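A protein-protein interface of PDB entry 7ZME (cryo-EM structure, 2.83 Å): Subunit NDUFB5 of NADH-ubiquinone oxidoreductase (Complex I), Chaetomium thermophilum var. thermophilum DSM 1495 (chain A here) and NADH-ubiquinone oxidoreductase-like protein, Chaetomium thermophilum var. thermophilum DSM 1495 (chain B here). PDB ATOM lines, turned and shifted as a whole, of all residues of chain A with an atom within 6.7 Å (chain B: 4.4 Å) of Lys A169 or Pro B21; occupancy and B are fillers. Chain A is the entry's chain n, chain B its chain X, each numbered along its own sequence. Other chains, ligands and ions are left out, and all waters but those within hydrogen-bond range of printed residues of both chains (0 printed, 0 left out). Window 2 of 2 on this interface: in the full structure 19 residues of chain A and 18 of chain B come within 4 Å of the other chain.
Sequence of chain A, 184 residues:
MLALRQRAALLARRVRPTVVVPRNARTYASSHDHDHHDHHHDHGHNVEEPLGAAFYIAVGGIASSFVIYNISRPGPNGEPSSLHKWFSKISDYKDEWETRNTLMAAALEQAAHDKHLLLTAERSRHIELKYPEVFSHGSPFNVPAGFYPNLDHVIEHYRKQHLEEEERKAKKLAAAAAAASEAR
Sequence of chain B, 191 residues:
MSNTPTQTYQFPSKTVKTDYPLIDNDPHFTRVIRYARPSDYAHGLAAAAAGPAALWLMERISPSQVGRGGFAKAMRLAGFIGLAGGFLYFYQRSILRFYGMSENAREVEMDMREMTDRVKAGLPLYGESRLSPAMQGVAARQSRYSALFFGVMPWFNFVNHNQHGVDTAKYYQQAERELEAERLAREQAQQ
OE2 of Glu A165 lies within hydrogen-bond range of N of Thr B18, 3.5 Å away. The side-chain hydroxyl (OG1) of Thr B18 sits at hydrogen-bond distance from the side-chain amino group (NZ) of Lys A169, at 2.8 Å. The backbone carbonyl oxygen (O) of Tyr B20 is in hydrogen-bond range of the side-chain amino group (NZ) of Lys A169, at 2.5 Å. The backbone NH of Leu B22 lies within hydrogen-bond range of the side-chain carboxylate of Glu A166 (3.2 Å).
OG1 of Thr B18 lies within hydrogen-bond range of O of Tyr B20. The side-chain hydroxyl (OG1) of Thr B18 sits at hydrogen-bond distance from the backbone carbonyl oxygen (O) of Gly B100 (3.2 Å). The backbone carbonyl oxygen of Gly B100 sits at hydrogen-bond distance from the backbone NH of Tyr B20, 3.0 Å away. The backbone carbonyl oxygen of Pro B21 sits at hydrogen-bond distance from the side-chain amide nitrogen of Asn B104 (2.7 Å). OE2 of Glu A165 is in salt-bridge range of NZ of Lys A169, at 3.9 Å. The side-chain amino group (NZ) of Lys A169 lies within salt-bridge range of the side-chain carboxylate (OE1) of Glu A166 (3.6 Å).
Among the printed residues, merely in contact across the chains: Glu A166 with Pro B21, Lys A169 with Pro B21 and Lys A169 with Leu B22.
Of the printed residues of chain B, Lys A169 touches Thr B18 (2.8 Å), Tyr B20 (2.5 Å), Pro B21 (3.98 Å) and Leu B22 (3.8 Å). Printed residues of chain A within 4 Å of Thr B18: Glu A165 and Lys A169. Printed residues of chain A within 4 Å of Tyr B20: Lys A169. Of the printed residues of chain A, Pro B21 touches Glu A166 (3.7 Å) and Lys A169 (3.98 Å). Printed residues of chain A within 4 Å of Leu B22: Glu A166 (3.2 Å) and Lys A169 (3.8 Å). The nearest printed residue of chain A that does not touch Pro B21 is Leu A173 (4.3 Å). The nearest printed residue of chain A that does not touch Tyr B20 is Glu A166 (4.8 Å).
Along chain B the printed residues that touch a printed residue of chain A span positions 18 to 22. Among the printed residues, 7 pairs touch across the chains. Among the printed residues, no Asp or Glu carboxylate lies within 4 Å of a Lys or Arg side-chain nitrogen of the other chain.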
ATOM      1  N   GLU A 164      -9.371 -21.867  -0.203  1.00  0.00           N
ATOM      2  CA  GLU A 164     -10.221 -21.937   0.982  1.00  0.00           C
ATOM      3  C   GLU A 164      -9.711 -22.973   1.976  1.00  0.00           C
ATOM      4  O   GLU A 164      -9.694 -22.725   3.185  1.00  0.00           O
ATOM      5  CB  GLU A 164     -11.664 -22.246   0.585  1.00  0.00           C
ATOM      6  CG  GLU A 164     -12.347 -21.147  -0.208  1.00  0.00           C
ATOM      7  CD  GLU A 164     -12.558 -19.888   0.610  1.00  0.00           C
ATOM      8  OE1 GLU A 164     -12.754 -20.003   1.839  1.00  0.00           O
ATOM      9  OE2 GLU A 164     -12.532 -18.784   0.026  1.00  0.00           O
ATOM     10  N   GLU A 165      -9.216 -24.114   1.529  1.00  0.00           N
ATOM     11  CA  GLU A 165      -8.762 -25.179   2.459  1.00  0.00           C
ATOM     12  C   GLU A 165      -7.506 -24.687   3.172  1.00  0.00           C
ATOM     13  O   GLU A 165      -7.452 -24.792   4.393  1.00  0.00           O
ATOM     14  CB  GLU A 165      -8.500 -26.467   1.678  1.00  0.00           C
ATOM     15  CG  GLU A 165      -7.612 -27.471   2.392  1.00  0.00           C
ATOM     16  CD  GLU A 165      -8.321 -28.448   3.314  1.00  0.00           C
ATOM     17  OE1 GLU A 165      -9.566 -28.505   3.273  1.00  0.00           O
ATOM     18  OE2 GLU A 165      -7.625 -29.148   4.075  1.00  0.00           O
ATOM     19  N   GLU A 166      -6.521 -24.208   2.415  1.00  0.00           N
ATOM     20  CA  GLU A 166      -5.242 -23.720   2.983  1.00  0.00           C
ATOM     21  C   GLU A 166      -5.486 -22.510   3.888  1.00  0.00           C
ATOM     22  O   GLU A 166      -4.825 -22.413   4.916  1.00  0.00           O
ATOM     23  CB  GLU A 166      -4.301 -23.364   1.832  1.00  0.00           C
ATOM     24  CG  GLU A 166      -4.054 -24.509   0.865  1.00  0.00           C
ATOM     25  CD  GLU A 166      -3.668 -25.860   1.448  1.00  0.00           C
ATOM     26  OE1 GLU A 166      -2.808 -25.900   2.352  1.00  0.00           O
ATOM     27  OE2 GLU A 166      -4.235 -26.875   0.993  1.00  0.00           O
ATOM     28  N   GLU A 167      -6.377 -21.613   3.485  1.00  0.00           N
ATOM     29  CA  GLU A 167      -6.725 -20.429   4.300  1.00  0.00           C
ATOM     30  C   GLU A 167      -7.297 -20.940   5.603  1.00  0.00           C
ATOM     31  O   GLU A 167      -6.889 -20.454   6.671  1.00  0.00           O
ATOM     32  CB  GLU A 167      -7.902 -19.712   3.652  1.00  0.00           C
ATOM     33  CG  GLU A 167      -8.365 -18.476   4.402  1.00  0.00           C
ATOM     34  CD  GLU A 167      -9.616 -17.851   3.812  1.00  0.00           C
ATOM     35  OE1 GLU A 167     -10.065 -18.328   2.751  1.00  0.00           O
ATOM     36  OE2 GLU A 167     -10.139 -16.894   4.417  1.00  0.00           O
ATOM     37  N   ARG A 168      -8.244 -21.861   5.493  1.00  0.00           N
ATOM     38  CA  ARG A 168      -8.874 -22.412   6.688  1.00  0.00           C
ATOM     39  C   ARG A 168      -7.849 -23.092   7.585  1.00  0.00           C
ATOM     40  O   ARG A 168      -7.917 -22.978   8.812  1.00  0.00           O
ATOM     41  CB  ARG A 168      -9.977 -23.391   6.292  1.00  0.00           C
ATOM     42  CG  ARG A 168     -10.937 -23.744   7.415  1.00  0.00           C
ATOM     43  CD  ARG A 168     -10.544 -25.059   8.055  1.00  0.00           C
ATOM     44  NE  ARG A 168     -10.037 -26.001   7.063  1.00  0.00           N
ATOM     45  CZ  ARG A 168      -9.224 -27.012   7.345  1.00  0.00           C
ATOM     46  NH1 ARG A 168      -8.816 -27.827   6.383  1.00  0.00           N
ATOM     47  NH2 ARG A 168      -8.823 -27.208   8.593  1.00  0.00           N
ATOM     48  N   LYS A 169      -6.904 -23.821   6.989  1.00  0.00           N
ATOM     49  CA  LYS A 169      -5.865 -24.464   7.786  1.00  0.00           C
ATOM     50  C   LYS A 169      -4.979 -23.431   8.467  1.00  0.00           C
ATOM     51  O   LYS A 169      -4.599 -23.599   9.630  1.00  0.00           O
ATOM     52  CB  LYS A 169      -5.031 -25.399   6.912  1.00  0.00           C
ATOM     53  CG  LYS A 169      -5.690 -26.738   6.654  1.00  0.00           C
ATOM     54  CD  LYS A 169      -4.695 -27.767   6.162  1.00  0.00           C
ATOM     55  CE  LYS A 169      -4.625 -27.788   4.648  1.00  0.00           C
ATOM     56  NZ  LYS A 169      -3.756 -28.889   4.161  1.00  0.00           N
ATOM     57  N   ALA A 170      -4.642 -22.354   7.756  1.00  0.00           N
ATOM     58  CA  ALA A 170      -3.778 -21.329   8.318  1.00  0.00           C
ATOM     59  C   ALA A 170      -4.402 -20.636   9.519  1.00  0.00           C
ATOM     60  O   ALA A 170      -3.670 -20.159  10.392  1.00  0.00           O
ATOM     61  CB  ALA A 170      -3.421 -20.296   7.248  1.00  0.00           C
ATOM     62  N   LYS A 171      -5.732 -20.565   9.584  1.00  0.00           N
ATOM     63  CA  LYS A 171      -6.384 -19.977  10.749  1.00  0.00           C
ATOM     64  C   LYS A 171      -6.331 -20.916  11.946  1.00  0.00           C
ATOM     65  O   LYS A 171      -6.112 -20.476  13.080  1.00  0.00           O
ATOM     66  CB  LYS A 171      -7.833 -19.612  10.416  1.00  0.00           C
ATOM     67  CG  LYS A 171      -7.991 -18.282   9.701  1.00  0.00           C
ATOM     68  CD  LYS A 171      -9.454 -17.878   9.596  1.00  0.00           C
ATOM     69  CE  LYS A 171     -10.202 -18.736   8.590  1.00  0.00           C
ATOM     70  NZ  LYS A 171     -11.616 -18.292   8.432  1.00  0.00           N
ATOM     71  N   LYS A 172      -6.540 -22.213  11.716  1.00  0.00           N
ATOM     72  CA  LYS A 172      -6.595 -23.162  12.823  1.00  0.00           C
ATOM     73  C   LYS A 172      -5.242 -23.298  13.511  1.00  0.00           C
ATOM     74  O   LYS A 172      -5.168 -23.357  14.743  1.00  0.00           O
ATOM     75  CB  LYS A 172      -7.083 -24.521  12.324  1.00  0.00           C
ATOM     76  CG  LYS A 172      -7.171 -25.583  13.404  1.00  0.00           C
ATOM     77  CD  LYS A 172      -7.556 -26.931  12.821  1.00  0.00           C
ATOM     78  CE  LYS A 172      -7.854 -27.941  13.918  1.00  0.00           C
ATOM     79  NZ  LYS A 172      -6.724 -28.066  14.878  1.00  0.00           N
ATOM     80  N   LEU A 173      -4.160 -23.352  12.732  1.00  0.00           N
ATOM     81  CA  LEU A 173      -2.836 -23.485  13.328  1.00  0.00           C
ATOM     82  C   LEU A 173      -2.438 -22.215  14.071  1.00  0.00           C
ATOM     83  O   LEU A 173      -1.727 -22.277  15.081  1.00  0.00           O
ATOM     84  CB  LEU A 173      -1.807 -23.842  12.253  1.00  0.00           C
ATOM     85  CG  LEU A 173      -1.604 -22.901  11.063  1.00  0.00           C
ATOM     86  CD1 LEU A 173      -0.519 -21.868  11.341  1.00  0.00           C
ATOM     87  CD2 LEU A 173      -1.274 -23.701   9.813  1.00  0.00           C
ATOM     88  N   ALA A 174      -2.882 -21.055  13.585  1.00  0.00           N
ATOM     89  CA  ALA A 174      -2.623 -19.811  14.301  1.00  0.00           C
ATOM     90  C   ALA A 174      -3.370 -19.766  15.627  1.00  0.00           C
ATOM     91  O   ALA A 174      -2.888 -19.155  16.587  1.00  0.00           O
ATOM     92  CB  ALA A 174      -3.002 -18.613  13.434  1.00  0.00           C
ATOM     93  N   THR B  18      -6.790 -32.242   5.396  1.00  0.00           N
ATOM     94  CA  THR B  18      -5.559 -32.687   6.109  1.00  0.00           C
ATOM     95  C   THR B  18      -5.302 -31.664   7.218  1.00  0.00           C
ATOM     96  O   THR B  18      -5.942 -30.610   7.153  1.00  0.00           O
ATOM     97  CB  THR B  18      -4.375 -32.931   5.156  1.00  0.00           C
ATOM     98  OG1 THR B  18      -3.939 -31.689   4.603  1.00  0.00           O
ATOM     99  CG2 THR B  18      -4.664 -33.908   4.039  1.00  0.00           C
ATOM    100  N   ASP B  19      -4.420 -31.937   8.181  1.00  0.00           N
ATOM    101  CA  ASP B  19      -4.253 -31.032   9.351  1.00  0.00           C
ATOM    102  C   ASP B  19      -3.134 -30.012   9.145  1.00  0.00           C
ATOM    103  O   ASP B  19      -3.054 -29.074   9.951  1.00  0.00           O
ATOM    104  CB  ASP B  19      -4.022 -31.831  10.631  1.00  0.00           C
ATOM    105  CG  ASP B  19      -5.112 -32.847  10.921  1.00  0.00           C
ATOM    106  OD1 ASP B  19      -6.225 -32.684  10.382  1.00  0.00           O
ATOM    107  OD2 ASP B  19      -4.837 -33.798  11.680  1.00  0.00           O
ATOM    108  N   TYR B  20      -2.320 -30.164   8.109  1.00  0.00           N
ATOM    109  CA  TYR B  20      -1.149 -29.268   7.930  1.00  0.00           C
ATOM    110  C   TYR B  20      -1.136 -28.707   6.507  1.00  0.00           C
ATOM    111  O   TYR B  20      -1.765 -29.300   5.642  1.00  0.00           O
ATOM    112  CB  TYR B  20       0.125 -30.025   8.298  1.00  0.00           C
ATOM    113  CG  TYR B  20       0.115 -30.613   9.685  1.00  0.00           C
ATOM    114  CD1 TYR B  20      -0.309 -31.912   9.910  1.00  0.00           C
ATOM    115  CD2 TYR B  20       0.514 -29.866  10.778  1.00  0.00           C
ATOM    116  CE1 TYR B  20      -0.332 -32.457  11.181  1.00  0.00           C
ATOM    117  CE2 TYR B  20       0.498 -30.395  12.056  1.00  0.00           C
ATOM    118  CZ  TYR B  20       0.077 -31.695  12.258  1.00  0.00           C
ATOM    119  OH  TYR B  20       0.064 -32.226  13.514  1.00  0.00           O
ATOM    120  N   PRO B  21      -0.411 -27.603   6.231  1.00  0.00           N
ATOM    121  CA  PRO B  21      -0.307 -27.035   4.880  1.00  0.00           C
ATOM    122  C   PRO B  21       0.203 -28.008   3.799  1.00  0.00           C
ATOM    123  O   PRO B  21       1.141 -28.713   4.063  1.00  0.00           O
ATOM    124  CB  PRO B  21       0.672 -25.868   5.083  1.00  0.00           C
ATOM    125  CG  PRO B  21       1.340 -26.120   6.403  1.00  0.00           C
ATOM    126  CD  PRO B  21       0.257 -26.770   7.228  1.00  0.00           C
ATOM    127  N   LEU B  22      -0.408 -28.009   2.606  1.00  0.00           N
ATOM    128  CA  LEU B  22       0.036 -28.881   1.495  1.00  0.00           C
ATOM    129  C   LEU B  22       1.185 -28.153   0.794  1.00  0.00           C
ATOM    130  O   LEU B  22       1.000 -26.990   0.419  1.00  0.00           O
ATOM    131  CB  LEU B  22      -1.139 -29.139   0.547  1.00  0.00           C
ATOM    132  CG  LEU B  22      -0.773 -29.594  -0.869  1.00  0.00           C
ATOM    133  CD1 LEU B  22      -0.350 -31.053  -0.894  1.00  0.00           C
ATOM    134  CD2 LEU B  22      -1.922 -29.366  -1.836  1.00  0.00           C
ATOM    135  N   ILE B  23       2.332 -28.816   0.653  1.00  0.00           N
ATOM    136  CA  ILE B  23       3.511 -28.201  -0.025  1.00  0.00           C
ATOM    137  C   ILE B  23       3.501 -28.701  -1.460  1.00  0.00           C
ATOM    138  O   ILE B  23       3.628 -27.889  -2.383  1.00  0.00           O
ATOM    139  CB  ILE B  23       4.803 -28.671   0.673  1.00  0.00           C
ATOM    140  CG1 ILE B  23       4.847 -28.274   2.148  1.00  0.00           C
ATOM    141  CG2 ILE B  23       6.039 -28.229  -0.084  1.00  0.00           C
ATOM    142  CD1 ILE B  23       5.877 -29.034   2.942  1.00  0.00           C
ATOM    143  N   ARG B  97       4.645 -35.296   5.068  1.00  0.00           N
ATOM    144  CA  ARG B  97       4.890 -33.873   5.426  1.00  0.00           C
ATOM    145  C   ARG B  97       4.689 -32.970   4.208  1.00  0.00           C
ATOM    146  O   ARG B  97       4.105 -31.895   4.368  1.00  0.00           O
ATOM    147  CB  ARG B  97       6.260 -33.715   6.082  1.00  0.00           C
ATOM    148  CG  ARG B  97       6.449 -34.630   7.280  1.00  0.00           C
ATOM    149  CD  ARG B  97       7.596 -34.253   8.184  1.00  0.00           C
ATOM    150  NE  ARG B  97       7.796 -35.315   9.151  1.00  0.00           N
ATOM    151  CZ  ARG B  97       8.671 -36.296   8.994  1.00  0.00           C
ATOM    152  NH1 ARG B  97       9.433 -36.322   7.917  1.00  0.00           N
ATOM    153  NH2 ARG B  97       8.793 -37.236   9.913  1.00  0.00           N
ATOM    154  N   GLY B 100       0.988 -32.512   3.789  1.00  0.00           N
ATOM    155  CA  GLY B 100       0.255 -31.834   4.871  1.00  0.00           C
ATOM    156  C   GLY B 100      -0.453 -32.834   5.747  1.00  0.00           C
ATOM    157  O   GLY B 100      -1.403 -32.447   6.433  1.00  0.00           O
ATOM    158  N   ASN B 104       4.670 -30.356   9.463  1.00  0.00           N
ATOM    159  CA  ASN B 104       5.659 -30.009   8.410  1.00  0.00           C
ATOM    160  C   ASN B 104       6.252 -28.603   8.514  1.00  0.00           C
ATOM    161  O   ASN B 104       6.677 -28.102   7.464  1.00  0.00           O
ATOM    162  CB  ASN B 104       5.011 -30.123   7.034  1.00  0.00           C
ATOM    163  CG  ASN B 104       3.714 -29.358   6.889  1.00  0.00           C
ATOM    164  OD1 ASN B 104       3.238 -28.731   7.830  1.00  0.00           O
ATOM    165  ND2 ASN B 104       3.134 -29.403   5.704  1.00  0.00           N
ATOM    166  N   VAL B 108       7.840 -26.837   5.350  1.00  0.00           N
ATOM    167  CA  VAL B 108       7.161 -25.626   4.813  1.00  0.00           C
ATOM    168  C   VAL B 108       8.169 -24.476   4.698  1.00  0.00           C
ATOM    169  O   VAL B 108       8.081 -23.736   3.708  1.00  0.00           O
ATOM    170  CB  VAL B 108       5.934 -25.261   5.669  1.00  0.00           C
ATOM    171  CG1 VAL B 108       5.254 -23.986   5.198  1.00  0.00           C
ATOM    172  CG2 VAL B 108       4.935 -26.401   5.735  1.00  0.00           C
